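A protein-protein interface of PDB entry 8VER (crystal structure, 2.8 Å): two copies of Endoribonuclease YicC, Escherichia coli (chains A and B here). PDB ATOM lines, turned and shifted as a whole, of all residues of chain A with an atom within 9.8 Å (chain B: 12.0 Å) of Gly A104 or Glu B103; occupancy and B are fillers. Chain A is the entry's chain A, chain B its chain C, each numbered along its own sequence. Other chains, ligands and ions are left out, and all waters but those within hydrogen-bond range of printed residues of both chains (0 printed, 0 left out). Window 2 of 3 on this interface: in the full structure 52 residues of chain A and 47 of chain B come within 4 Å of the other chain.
The backbone NH of Ile A106 sits at hydrogen-bond distance from the side-chain carboxylate of Glu B103. The side-chain carboxylate of Glu A105 sits at hydrogen-bond distance from the backbone NH of Gly B104 (3.1 Å). OE2 of Glu B103 lies within salt-bridge range of NZ of Lys A98, 2.5 Å away.
The backbone carbonyl oxygen of Lys B98 lies within hydrogen-bond range of the backbone NH of Glu B103 (3.4 Å). N of Glu A103 sits at hydrogen-bond distance from O of Lys A98. OG of Ser B101 is in hydrogen-bond range of O of Glu B103 (2.8 Å). The side-chain amide oxygen (OD1) of Asn B95 lies close to the side-chain amino group (NZ) of Lys B98 (3.3 Å). The backbone carbonyl oxygen (O) of Val A91 sits at hydrogen-bond distance from the side-chain amide nitrogen (ND2) of Asn A95. The side-chain amide oxygen of Asn A95 is in hydrogen-bond range of the side-chain amino group of Lys A98 (3.1 Å).
Among the printed residues, merely in contact across the chains: Val A91 with Ser B101 (3.8 Å), Gly A104 with Glu B103 (3.9 Å), Glu A105 with Glu B103 (3.4 Å), Ile A106 with Ser B101 (3.99 Å), Ile A106 with Gly B104 (3.4 Å), Asn A107 with Glu B105 (3.5 Å), Pro A108 with Ala B94 (3.5 Å), Pro A108 with Val B97 (3.8 Å), Pro A108 with Lys B98 (3.7 Å), Pro A108 with Glu B105 (3.7 Å) and Ile A111 with Val B97 (3.9 Å).
Gly A104 touches just one residue of chain B: Glu B103. Glu B103 touches just these residues of chain A: Lys A98 (2.5 Å), Gly A104 (3.9 Å), Glu A105 (3.4 Å) and Ile A106 (3.1 Å). Printed residues of chain B within 4 Å of Lys A98: Glu B103 (2.5 Å). No residue of chain B comes within 4 Å of Ser A101. No residue of chain B comes within 4 Å of Glu A103. Glu A105 touches just these residues of chain B: Glu B103 (3.4 Å) and Gly B104 (3.1 Å). Of chain A, only Glu A105 and Ile A106 come within 4 Å of Gly B104. Printed residues of chain A within 4 Å of Ala B94: Pro A108. Of the printed residues of chain A, Glu B105 touches Asn A107 and Pro A108. Of the printed residues of chain B, Ile A106 touches Ser B101, Glu B103 and Gly B104. Of the printed residues of chain B, Asn A107 touches Glu B105. Of the printed residues of chain B, Pro A108 touches Ala B94, Val B97, Lys B98 and Glu B105.
Printed residues of chain B that touch a printed residue of chain A: Ala B94, Val B97, Lys B98, Ser B101, Glu B103, Gly B104 and Glu B105. Of the 19 printed residues of chain A, 8 touch a printed residue of chain B. Among the printed residues, 14 pairs touch across the chains. Among the printed residues, Asp or Glu carboxylates within 4 Å of a Lys or Arg side-chain nitrogen of the other chain: Lys A98 with Glu B103 (2.5 Å).
Gly A104 touches Glu B103, but with the chains exchanged Glu A103 does not touch Gly B104 (11.5 Å). Ile A106 touches Ser B101, but with the chains exchanged Ser A101 does not touch Ile B106 (19.3 Å). Ile A106 touches Gly B104, but with the chains exchanged Gly A104 does not touch Ile B106 (13.2 Å). Asn A107 touches Glu B105, but with the chains exchanged Glu A105 does not touch Asn B107 (10.1 Å). 15 positions are printed for both chains. Of the 14 pairs that touch across the chains among the printed residues, none has its exchanged pair printed and touching as well.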
ATOM      1  N   LEU A  90      16.764   2.969   3.592  1.00  0.00           N
ATOM      2  CA  LEU A  90      17.596   3.305   2.441  1.00  0.00           C
ATOM      3  C   LEU A  90      18.579   2.185   2.126  1.00  0.00           C
ATOM      4  O   LEU A  90      18.866   1.915   0.953  1.00  0.00           O
ATOM      5  CB  LEU A  90      18.339   4.615   2.694  1.00  0.00           C
ATOM      6  CG  LEU A  90      17.464   5.857   2.863  1.00  0.00           C
ATOM      7  CD1 LEU A  90      18.312   7.055   3.249  1.00  0.00           C
ATOM      8  CD2 LEU A  90      16.686   6.141   1.590  1.00  0.00           C
ATOM      9  N   VAL A  91      19.110   1.527   3.158  1.00  0.00           N
ATOM     10  CA  VAL A  91      20.025   0.410   2.937  1.00  0.00           C
ATOM     11  C   VAL A  91      19.292  -0.761   2.296  1.00  0.00           C
ATOM     12  O   VAL A  91      19.824  -1.430   1.400  1.00  0.00           O
ATOM     13  CB  VAL A  91      20.699   0.004   4.261  1.00  0.00           C
ATOM     14  CG1 VAL A  91      21.523  -1.264   4.081  1.00  0.00           C
ATOM     15  CG2 VAL A  91      21.572   1.135   4.775  1.00  0.00           C
ATOM     16  N   ALA A  94      18.726   0.189  -1.296  1.00  0.00           N
ATOM     17  CA  ALA A  94      19.969   0.109  -2.058  1.00  0.00           C
ATOM     18  C   ALA A  94      20.370  -1.339  -2.303  1.00  0.00           C
ATOM     19  O   ALA A  94      20.940  -1.663  -3.352  1.00  0.00           O
ATOM     20  CB  ALA A  94      21.083   0.860  -1.331  1.00  0.00           C
ATOM     21  N   ASN A  95      20.082  -2.225  -1.346  1.00  0.00           N
ATOM     22  CA  ASN A  95      20.344  -3.646  -1.549  1.00  0.00           C
ATOM     23  C   ASN A  95      19.548  -4.189  -2.728  1.00  0.00           C
ATOM     24  O   ASN A  95      20.046  -5.025  -3.491  1.00  0.00           O
ATOM     25  CB  ASN A  95      20.014  -4.429  -0.277  1.00  0.00           C
ATOM     26  CG  ASN A  95      21.049  -4.236   0.813  1.00  0.00           C
ATOM     27  OD1 ASN A  95      22.240  -4.103   0.537  1.00  0.00           O
ATOM     28  ND2 ASN A  95      20.597  -4.225   2.062  1.00  0.00           N
ATOM     29  N   TRP A  96      18.306  -3.727  -2.890  1.00  0.00           N
ATOM     30  CA  TRP A  96      17.501  -4.154  -4.029  1.00  0.00           C
ATOM     31  C   TRP A  96      18.115  -3.690  -5.342  1.00  0.00           C
ATOM     32  O   TRP A  96      18.115  -4.428  -6.334  1.00  0.00           O
ATOM     33  CB  TRP A  96      16.073  -3.626  -3.894  1.00  0.00           C
ATOM     34  CG  TRP A  96      15.193  -4.011  -5.040  1.00  0.00           C
ATOM     35  CD1 TRP A  96      14.431  -5.137  -5.143  1.00  0.00           C
ATOM     36  CD2 TRP A  96      14.988  -3.276  -6.252  1.00  0.00           C
ATOM     37  NE1 TRP A  96      13.763  -5.148  -6.343  1.00  0.00           N
ATOM     38  CE2 TRP A  96      14.088  -4.016  -7.042  1.00  0.00           C
ATOM     39  CE3 TRP A  96      15.479  -2.063  -6.744  1.00  0.00           C
ATOM     40  CZ2 TRP A  96      13.667  -3.583  -8.297  1.00  0.00           C
ATOM     41  CZ3 TRP A  96      15.060  -1.636  -7.990  1.00  0.00           C
ATOM     42  CH2 TRP A  96      14.163  -2.393  -8.752  1.00  0.00           C
ATOM     43  N   VAL A  97      18.635  -2.460  -5.370  1.00  0.00           N
ATOM     44  CA  VAL A  97      19.304  -1.964  -6.569  1.00  0.00           C
ATOM     45  C   VAL A  97      20.564  -2.772  -6.840  1.00  0.00           C
ATOM     46  O   VAL A  97      20.917  -3.031  -7.997  1.00  0.00           O
ATOM     47  CB  VAL A  97      19.611  -0.461  -6.427  1.00  0.00           C
ATOM     48  CG1 VAL A  97      20.335   0.063  -7.659  1.00  0.00           C
ATOM     49  CG2 VAL A  97      18.329   0.319  -6.187  1.00  0.00           C
ATOM     50  N   LYS A  98      21.251  -3.199  -5.779  1.00  0.00           N
ATOM     51  CA  LYS A  98      22.498  -3.933  -5.958  1.00  0.00           C
ATOM     52  C   LYS A  98      22.270  -5.299  -6.590  1.00  0.00           C
ATOM     53  O   LYS A  98      23.156  -5.806  -7.284  1.00  0.00           O
ATOM     54  CB  LYS A  98      23.225  -4.082  -4.623  1.00  0.00           C
ATOM     55  CG  LYS A  98      24.076  -2.879  -4.258  1.00  0.00           C
ATOM     56  CD  LYS A  98      25.003  -3.194  -3.102  1.00  0.00           C
ATOM     57  CE  LYS A  98      24.210  -3.564  -1.867  1.00  0.00           C
ATOM     58  NZ  LYS A  98      25.091  -3.896  -0.717  1.00  0.00           N
ATOM     59  N   MET A  99      21.106  -5.912  -6.364  1.00  0.00           N
ATOM     60  CA  MET A  99      20.827  -7.196  -6.996  1.00  0.00           C
ATOM     61  C   MET A  99      20.332  -7.038  -8.427  1.00  0.00           C
ATOM     62  O   MET A  99      20.435  -7.988  -9.211  1.00  0.00           O
ATOM     63  CB  MET A  99      19.810  -7.992  -6.172  1.00  0.00           C
ATOM     64  CG  MET A  99      18.351  -7.651  -6.434  1.00  0.00           C
ATOM     65  SD  MET A  99      17.253  -8.776  -5.545  1.00  0.00           S
ATOM     66  CE  MET A  99      15.651  -8.243  -6.145  1.00  0.00           C
ATOM     67  N   GLN A 100      19.801  -5.867  -8.785  1.00  0.00           N
ATOM     68  CA  GLN A 100      19.456  -5.613 -10.179  1.00  0.00           C
ATOM     69  C   GLN A 100      20.701  -5.306 -11.001  1.00  0.00           C
ATOM     70  O   GLN A 100      20.847  -5.795 -12.127  1.00  0.00           O
ATOM     71  CB  GLN A 100      18.457  -4.461 -10.275  1.00  0.00           C
ATOM     72  CG  GLN A 100      17.132  -4.718  -9.582  1.00  0.00           C
ATOM     73  CD  GLN A 100      16.323  -5.809 -10.251  1.00  0.00           C
ATOM     74  OE1 GLN A 100      16.529  -6.121 -11.425  1.00  0.00           O
ATOM     75  NE2 GLN A 100      15.397  -6.399  -9.507  1.00  0.00           N
ATOM     76  N   SER A 101      21.607  -4.497 -10.453  1.00  0.00           N
ATOM     77  CA  SER A 101      22.844  -4.166 -11.147  1.00  0.00           C
ATOM     78  C   SER A 101      23.925  -5.219 -10.947  1.00  0.00           C
ATOM     79  O   SER A 101      24.904  -5.230 -11.701  1.00  0.00           O
ATOM     80  CB  SER A 101      23.363  -2.806 -10.677  1.00  0.00           C
ATOM     81  OG  SER A 101      23.683  -2.831  -9.297  1.00  0.00           O
ATOM     82  N   ASP A 102      23.770  -6.091  -9.949  1.00  0.00           N
ATOM     83  CA  ASP A 102      24.728  -7.147  -9.628  1.00  0.00           C
ATOM     84  C   ASP A 102      26.093  -6.590  -9.234  1.00  0.00           C
ATOM     85  O   ASP A 102      27.107  -7.284  -9.357  1.00  0.00           O
ATOM     86  CB  ASP A 102      24.879  -8.138 -10.788  1.00  0.00           C
ATOM     87  CG  ASP A 102      25.178  -9.542 -10.314  1.00  0.00           C
ATOM     88  OD1 ASP A 102      24.989  -9.808  -9.108  1.00  0.00           O
ATOM     89  OD2 ASP A 102      25.601 -10.376 -11.141  1.00  0.00           O
ATOM     90  N   GLU A 103      26.135  -5.352  -8.750  1.00  0.00           N
ATOM     91  CA  GLU A 103      27.383  -4.700  -8.376  1.00  0.00           C
ATOM     92  C   GLU A 103      27.052  -3.456  -7.558  1.00  0.00           C
ATOM     93  O   GLU A 103      25.898  -3.028  -7.482  1.00  0.00           O
ATOM     94  CB  GLU A 103      28.217  -4.333  -9.606  1.00  0.00           C
ATOM     95  CG  GLU A 103      27.502  -3.402 -10.573  1.00  0.00           C
ATOM     96  CD  GLU A 103      28.320  -3.103 -11.813  1.00  0.00           C
ATOM     97  OE1 GLU A 103      29.517  -3.461 -11.839  1.00  0.00           O
ATOM     98  OE2 GLU A 103      27.766  -2.513 -12.764  1.00  0.00           O
ATOM     99  N   GLY A 104      28.081  -2.885  -6.951  1.00  0.00           N
ATOM    100  CA  GLY A 104      27.948  -1.659  -6.193  1.00  0.00           C
ATOM    101  C   GLY A 104      28.227  -1.871  -4.713  1.00  0.00           C
ATOM    102  O   GLY A 104      28.164  -2.982  -4.181  1.00  0.00           O
ATOM    103  N   GLU A 105      28.545  -0.764  -4.039  1.00  0.00           N
ATOM    104  CA  GLU A 105      28.814  -0.768  -2.608  1.00  0.00           C
ATOM    105  C   GLU A 105      28.162   0.452  -1.974  1.00  0.00           C
ATOM    106  O   GLU A 105      28.237   1.558  -2.518  1.00  0.00           O
ATOM    107  CB  GLU A 105      30.323  -0.781  -2.317  1.00  0.00           C
ATOM    108  CG  GLU A 105      30.679  -1.119  -0.872  1.00  0.00           C
ATOM    109  CD  GLU A 105      32.177  -1.222  -0.642  1.00  0.00           C
ATOM    110  OE1 GLU A 105      32.944  -0.652  -1.445  1.00  0.00           O
ATOM    111  OE2 GLU A 105      32.586  -1.879   0.340  1.00  0.00           O
ATOM    112  N   ILE A 106      27.527   0.244  -0.823  1.00  0.00           N
ATOM    113  CA  ILE A 106      26.788   1.302  -0.140  1.00  0.00           C
ATOM    114  C   ILE A 106      27.778   2.172   0.629  1.00  0.00           C
ATOM    115  O   ILE A 106      28.403   1.719   1.591  1.00  0.00           O
ATOM    116  CB  ILE A 106      25.720   0.726   0.795  1.00  0.00           C
ATOM    117  CG1 ILE A 106      24.690  -0.078   0.000  1.00  0.00           C
ATOM    118  CG2 ILE A 106      25.042   1.841   1.579  1.00  0.00           C
ATOM    119  CD1 ILE A 106      23.633  -0.730   0.860  1.00  0.00           C
ATOM    120  N   ASN A 107      27.911   3.424   0.211  1.00  0.00           N
ATOM    121  CA  ASN A 107      28.765   4.372   0.914  1.00  0.00           C
ATOM    122  C   ASN A 107      28.047   4.875   2.161  1.00  0.00           C
ATOM    123  O   ASN A 107      26.937   5.408   2.050  1.00  0.00           O
ATOM    124  CB  ASN A 107      29.124   5.539   0.000  1.00  0.00           C
ATOM    125  CG  ASN A 107      30.307   6.343   0.507  1.00  0.00           C
ATOM    126  OD1 ASN A 107      30.477   6.537   1.711  1.00  0.00           O
ATOM    127  ND2 ASN A 107      31.133   6.819  -0.416  1.00  0.00           N
ATOM    128  N   PRO A 108      28.629   4.723   3.353  1.00  0.00           N
ATOM    129  CA  PRO A 108      27.919   5.159   4.568  1.00  0.00           C
ATOM    130  C   PRO A 108      27.663   6.655   4.621  1.00  0.00           C
ATOM    131  O   PRO A 108      26.573   7.076   5.030  1.00  0.00           O
ATOM    132  CB  PRO A 108      28.851   4.699   5.699  1.00  0.00           C
ATOM    133  CG  PRO A 108      30.197   4.566   5.057  1.00  0.00           C
ATOM    134  CD  PRO A 108      29.927   4.099   3.661  1.00  0.00           C
ATOM    135  N   VAL A 109      28.639   7.473   4.219  1.00  0.00           N
ATOM    136  CA  VAL A 109      28.461   8.921   4.261  1.00  0.00           C
ATOM    137  C   VAL A 109      27.352   9.356   3.313  1.00  0.00           C
ATOM    138  O   VAL A 109      26.617  10.309   3.599  1.00  0.00           O
ATOM    139  CB  VAL A 109      29.795   9.628   3.946  1.00  0.00           C
ATOM    140  CG1 VAL A 109      29.612  11.137   3.891  1.00  0.00           C
ATOM    141  CG2 VAL A 109      30.840   9.258   4.987  1.00  0.00           C
ATOM    142  N   ILE A 111      24.640   7.767   2.773  1.00  0.00           N
ATOM    143  CA  ILE A 111      23.391   7.563   3.497  1.00  0.00           C
ATOM    144  C   ILE A 111      23.160   8.696   4.488  1.00  0.00           C
ATOM    145  O   ILE A 111      22.022   9.138   4.697  1.00  0.00           O
ATOM    146  CB  ILE A 111      23.400   6.191   4.196  1.00  0.00           C
ATOM    147  CG1 ILE A 111      23.557   5.075   3.165  1.00  0.00           C
ATOM    148  CG2 ILE A 111      22.121   5.984   4.991  1.00  0.00           C
ATOM    149  CD1 ILE A 111      22.361   4.927   2.255  1.00  0.00           C
ATOM    150  N   VAL B  91      32.138   9.899  12.241  1.00  0.00           N
ATOM    151  CA  VAL B  91      32.761   8.611  11.948  1.00  0.00           C
ATOM    152  C   VAL B  91      32.044   7.490  12.688  1.00  0.00           C
ATOM    153  O   VAL B  91      31.806   6.412  12.129  1.00  0.00           O
ATOM    154  CB  VAL B  91      34.262   8.658  12.290  1.00  0.00           C
ATOM    155  CG1 VAL B  91      34.870   7.269  12.215  1.00  0.00           C
ATOM    156  CG2 VAL B  91      34.985   9.606  11.345  1.00  0.00           C
ATOM    157  N   THR B  92      31.679   7.722  13.953  1.00  0.00           N
ATOM    158  CA  THR B  92      30.942   6.710  14.705  1.00  0.00           C
ATOM    159  C   THR B  92      29.544   6.507  14.134  1.00  0.00           C
ATOM    160  O   THR B  92      29.026   5.384  14.129  1.00  0.00           O
ATOM    161  CB  THR B  92      30.866   7.100  16.181  1.00  0.00           C
ATOM    162  OG1 THR B  92      30.291   8.406  16.305  1.00  0.00           O
ATOM    163  CG2 THR B  92      32.255   7.106  16.803  1.00  0.00           C
ATOM    164  N   ALA B  93      28.915   7.581  13.651  1.00  0.00           N
ATOM    165  CA  ALA B  93      27.613   7.440  13.007  1.00  0.00           C
ATOM    166  C   ALA B  93      27.728   6.670  11.698  1.00  0.00           C
ATOM    167  O   ALA B  93      26.860   5.852  11.375  1.00  0.00           O
ATOM    168  CB  ALA B  93      26.987   8.814  12.773  1.00  0.00           C
ATOM    169  N   ALA B  94      28.796   6.915  10.933  1.00  0.00           N
ATOM    170  CA  ALA B  94      28.990   6.179   9.690  1.00  0.00           C
ATOM    171  C   ALA B  94      29.328   4.718   9.955  1.00  0.00           C
ATOM    172  O   ALA B  94      28.994   3.849   9.141  1.00  0.00           O
ATOM    173  CB  ALA B  94      30.084   6.837   8.852  1.00  0.00           C
ATOM    174  N   ASN B  95      29.985   4.428  11.081  1.00  0.00           N
ATOM    175  CA  ASN B  95      30.257   3.040  11.442  1.00  0.00           C
ATOM    176  C   ASN B  95      28.963   2.264  11.645  1.00  0.00           C
ATOM    177  O   ASN B  95      28.880   1.079  11.300  1.00  0.00           O
ATOM    178  CB  ASN B  95      31.116   2.980  12.706  1.00  0.00           C
ATOM    179  CG  ASN B  95      32.534   3.463  12.473  1.00  0.00           C
ATOM    180  OD1 ASN B  95      33.015   3.490  11.341  1.00  0.00           O
ATOM    181  ND2 ASN B  95      33.215   3.840  13.550  1.00  0.00           N
ATOM    182  N   TRP B  96      27.942   2.915  12.208  1.00  0.00           N
ATOM    183  CA  TRP B  96      26.652   2.259  12.383  1.00  0.00           C
ATOM    184  C   TRP B  96      26.031   1.908  11.038  1.00  0.00           C
ATOM    185  O   TRP B  96      25.463   0.822  10.870  1.00  0.00           O
ATOM    186  CB  TRP B  96      25.713   3.155  13.189  1.00  0.00           C
ATOM    187  CG  TRP B  96      24.378   2.532  13.469  1.00  0.00           C
ATOM    188  CD1 TRP B  96      24.044   1.758  14.542  1.00  0.00           C
ATOM    189  CD2 TRP B  96      23.196   2.634  12.665  1.00  0.00           C
ATOM    190  NE1 TRP B  96      22.729   1.370  14.455  1.00  0.00           N
ATOM    191  CE2 TRP B  96      22.186   1.894  13.312  1.00  0.00           C
ATOM    192  CE3 TRP B  96      22.895   3.276  11.460  1.00  0.00           C
ATOM    193  CZ2 TRP B  96      20.898   1.780  12.795  1.00  0.00           C
ATOM    194  CZ3 TRP B  96      21.616   3.162  10.949  1.00  0.00           C
ATOM    195  CH2 TRP B  96      20.633   2.419  11.616  1.00  0.00           C
ATOM    196  N   VAL B  97      26.127   2.818  10.067  1.00  0.00           N
ATOM    197  CA  VAL B  97      25.609   2.539   8.731  1.00  0.00           C
ATOM    198  C   VAL B  97      26.393   1.403   8.089  1.00  0.00           C
ATOM    199  O   VAL B  97      25.826   0.556   7.387  1.00  0.00           O
ATOM    200  CB  VAL B  97      25.644   3.814   7.868  1.00  0.00           C
ATOM    201  CG1 VAL B  97      25.019   3.554   6.505  1.00  0.00           C
ATOM    202  CG2 VAL B  97      24.929   4.954   8.579  1.00  0.00           C
ATOM    203  N   LYS B  98      27.707   1.362   8.324  1.00  0.00           N
ATOM    204  CA  LYS B  98      28.510   0.264   7.800  1.00  0.00           C
ATOM    205  C   LYS B  98      28.095  -1.068   8.408  1.00  0.00           C
ATOM    206  O   LYS B  98      28.184  -2.107   7.746  1.00  0.00           O
ATOM    207  CB  LYS B  98      29.995   0.515   8.058  1.00  0.00           C
ATOM    208  CG  LYS B  98      30.588   1.661   7.259  1.00  0.00           C
ATOM    209  CD  LYS B  98      32.105   1.642   7.336  1.00  0.00           C
ATOM    210  CE  LYS B  98      32.571   1.623   8.779  1.00  0.00           C
ATOM    211  NZ  LYS B  98      34.052   1.543   8.892  1.00  0.00           N
ATOM    212  N   MET B  99      27.642  -1.060   9.663  1.00  0.00           N
ATOM    213  CA  MET B  99      27.214  -2.304  10.294  1.00  0.00           C
ATOM    214  C   MET B  99      25.895  -2.792   9.709  1.00  0.00           C
ATOM    215  O   MET B  99      25.685  -4.002   9.558  1.00  0.00           O
ATOM    216  CB  MET B  99      27.097  -2.115  11.805  1.00  0.00           C
ATOM    217  CG  MET B  99      26.699  -3.371  12.558  1.00  0.00           C
ATOM    218  SD  MET B  99      26.675  -3.108  14.341  1.00  0.00           S
ATOM    219  CE  MET B  99      25.496  -1.764  14.460  1.00  0.00           C
ATOM    220  N   GLN B 100      24.995  -1.867   9.370  1.00  0.00           N
ATOM    221  CA  GLN B 100      23.734  -2.256   8.746  1.00  0.00           C
ATOM    222  C   GLN B 100      23.962  -2.753   7.323  1.00  0.00           C
ATOM    223  O   GLN B 100      23.465  -3.819   6.938  1.00  0.00           O
ATOM    224  CB  GLN B 100      22.759  -1.079   8.759  1.00  0.00           C
ATOM    225  CG  GLN B 100      22.547  -0.465  10.133  1.00  0.00           C
ATOM    226  CD  GLN B 100      21.998  -1.461  11.133  1.00  0.00           C
ATOM    227  OE1 GLN B 100      21.127  -2.268  10.807  1.00  0.00           O
ATOM    228  NE2 GLN B 100      22.511  -1.415  12.358  1.00  0.00           N
ATOM    229  N   SER B 101      24.716  -1.991   6.528  1.00  0.00           N
ATOM    230  CA  SER B 101      24.989  -2.382   5.151  1.00  0.00           C
ATOM    231  C   SER B 101      25.991  -3.526   5.061  1.00  0.00           C
ATOM    232  O   SER B 101      26.057  -4.195   4.024  1.00  0.00           O
ATOM    233  CB  SER B 101      25.500  -1.174   4.360  1.00  0.00           C
ATOM    234  OG  SER B 101      26.658  -0.620   4.964  1.00  0.00           O
ATOM    235  N   ASP B 102      26.765  -3.764   6.123  1.00  0.00           N
ATOM    236  CA  ASP B 102      27.809  -4.788   6.174  1.00  0.00           C
ATOM    237  C   ASP B 102      28.904  -4.545   5.142  1.00  0.00           C
ATOM    238  O   ASP B 102      29.631  -5.475   4.775  1.00  0.00           O
ATOM    239  CB  ASP B 102      27.231  -6.199   6.003  1.00  0.00           C
ATOM    240  CG  ASP B 102      27.881  -7.211   6.930  1.00  0.00           C
ATOM    241  OD1 ASP B 102      28.806  -6.826   7.675  1.00  0.00           O
ATOM    242  OD2 ASP B 102      27.460  -8.387   6.919  1.00  0.00           O
ATOM    243  N   GLU B 103      29.037  -3.308   4.668  1.00  0.00           N
ATOM    244  CA  GLU B 103      30.043  -2.952   3.675  1.00  0.00           C
ATOM    245  C   GLU B 103      30.173  -1.436   3.655  1.00  0.00           C
ATOM    246  O   GLU B 103      29.387  -0.719   4.279  1.00  0.00           O
ATOM    247  CB  GLU B 103      29.680  -3.492   2.285  1.00  0.00           C
ATOM    248  CG  GLU B 103      28.398  -2.903   1.707  1.00  0.00           C
ATOM    249  CD  GLU B 103      28.103  -3.403   0.305  1.00  0.00           C
ATOM    250  OE1 GLU B 103      28.695  -4.425  -0.101  1.00  0.00           O
ATOM    251  OE2 GLU B 103      27.280  -2.773  -0.393  1.00  0.00           O
ATOM    252  N   GLY B 104      31.174  -0.957   2.932  1.00  0.00           N
ATOM    253  CA  GLY B 104      31.394   0.464   2.755  1.00  0.00           C
ATOM    254  C   GLY B 104      32.730   0.916   3.311  1.00  0.00           C
ATOM    255  O   GLY B 104      33.420   0.199   4.038  1.00  0.00           O
ATOM    256  N   GLU B 105      33.084   2.145   2.944  1.00  0.00           N
ATOM    257  CA  GLU B 105      34.324   2.766   3.383  1.00  0.00           C
ATOM    258  C   GLU B 105      34.085   4.257   3.560  1.00  0.00           C
ATOM    259  O   GLU B 105      33.431   4.891   2.725  1.00  0.00           O
ATOM    260  CB  GLU B 105      35.460   2.521   2.382  1.00  0.00           C
ATOM    261  CG  GLU B 105      36.834   2.929   2.887  1.00  0.00           C
ATOM    262  CD  GLU B 105      37.939   2.590   1.907  1.00  0.00           C
ATOM    263  OE1 GLU B 105      37.642   2.442   0.703  1.00  0.00           O
ATOM    264  OE2 GLU B 105      39.104   2.466   2.342  1.00  0.00           O
ATOM    265  N   ILE B 106      34.612   4.808   4.649  1.00  0.00           N
ATOM    266  CA  ILE B 106      34.429   6.221   4.966  1.00  0.00           C
ATOM    267  C   ILE B 106      35.457   7.043   4.195  1.00  0.00           C
ATOM    268  O   ILE B 106      36.666   6.834   4.339  1.00  0.00           O
ATOM    269  CB  ILE B 106      34.550   6.468   6.476  1.00  0.00           C
ATOM    270  CG1 ILE B 106      33.472   5.697   7.241  1.00  0.00           C
ATOM    271  CG2 ILE B 106      34.475   7.959   6.782  1.00  0.00           C
ATOM    272  CD1 ILE B 106      33.598   5.818   8.744  1.00  0.00           C
ATOM    273  N   ASN B 107      34.974   7.982   3.382  1.00  0.00           N
ATOM    274  CA  ASN B 107      35.847   8.892   2.646  1.00  0.00           C
ATOM    275  C   ASN B 107      36.246  10.055   3.547  1.00  0.00           C
ATOM    276  O   ASN B 107      35.367  10.757   4.060  1.00  0.00           O
ATOM    277  CB  ASN B 107      35.148   9.411   1.392  1.00  0.00           C
ATOM    278  CG  ASN B 107      36.113  10.032   0.395  1.00  0.00           C
ATOM    279  OD1 ASN B 107      37.053  10.731   0.771  1.00  0.00           O
ATOM    280  ND2 ASN B 107      35.887   9.770  -0.888  1.00  0.00           N
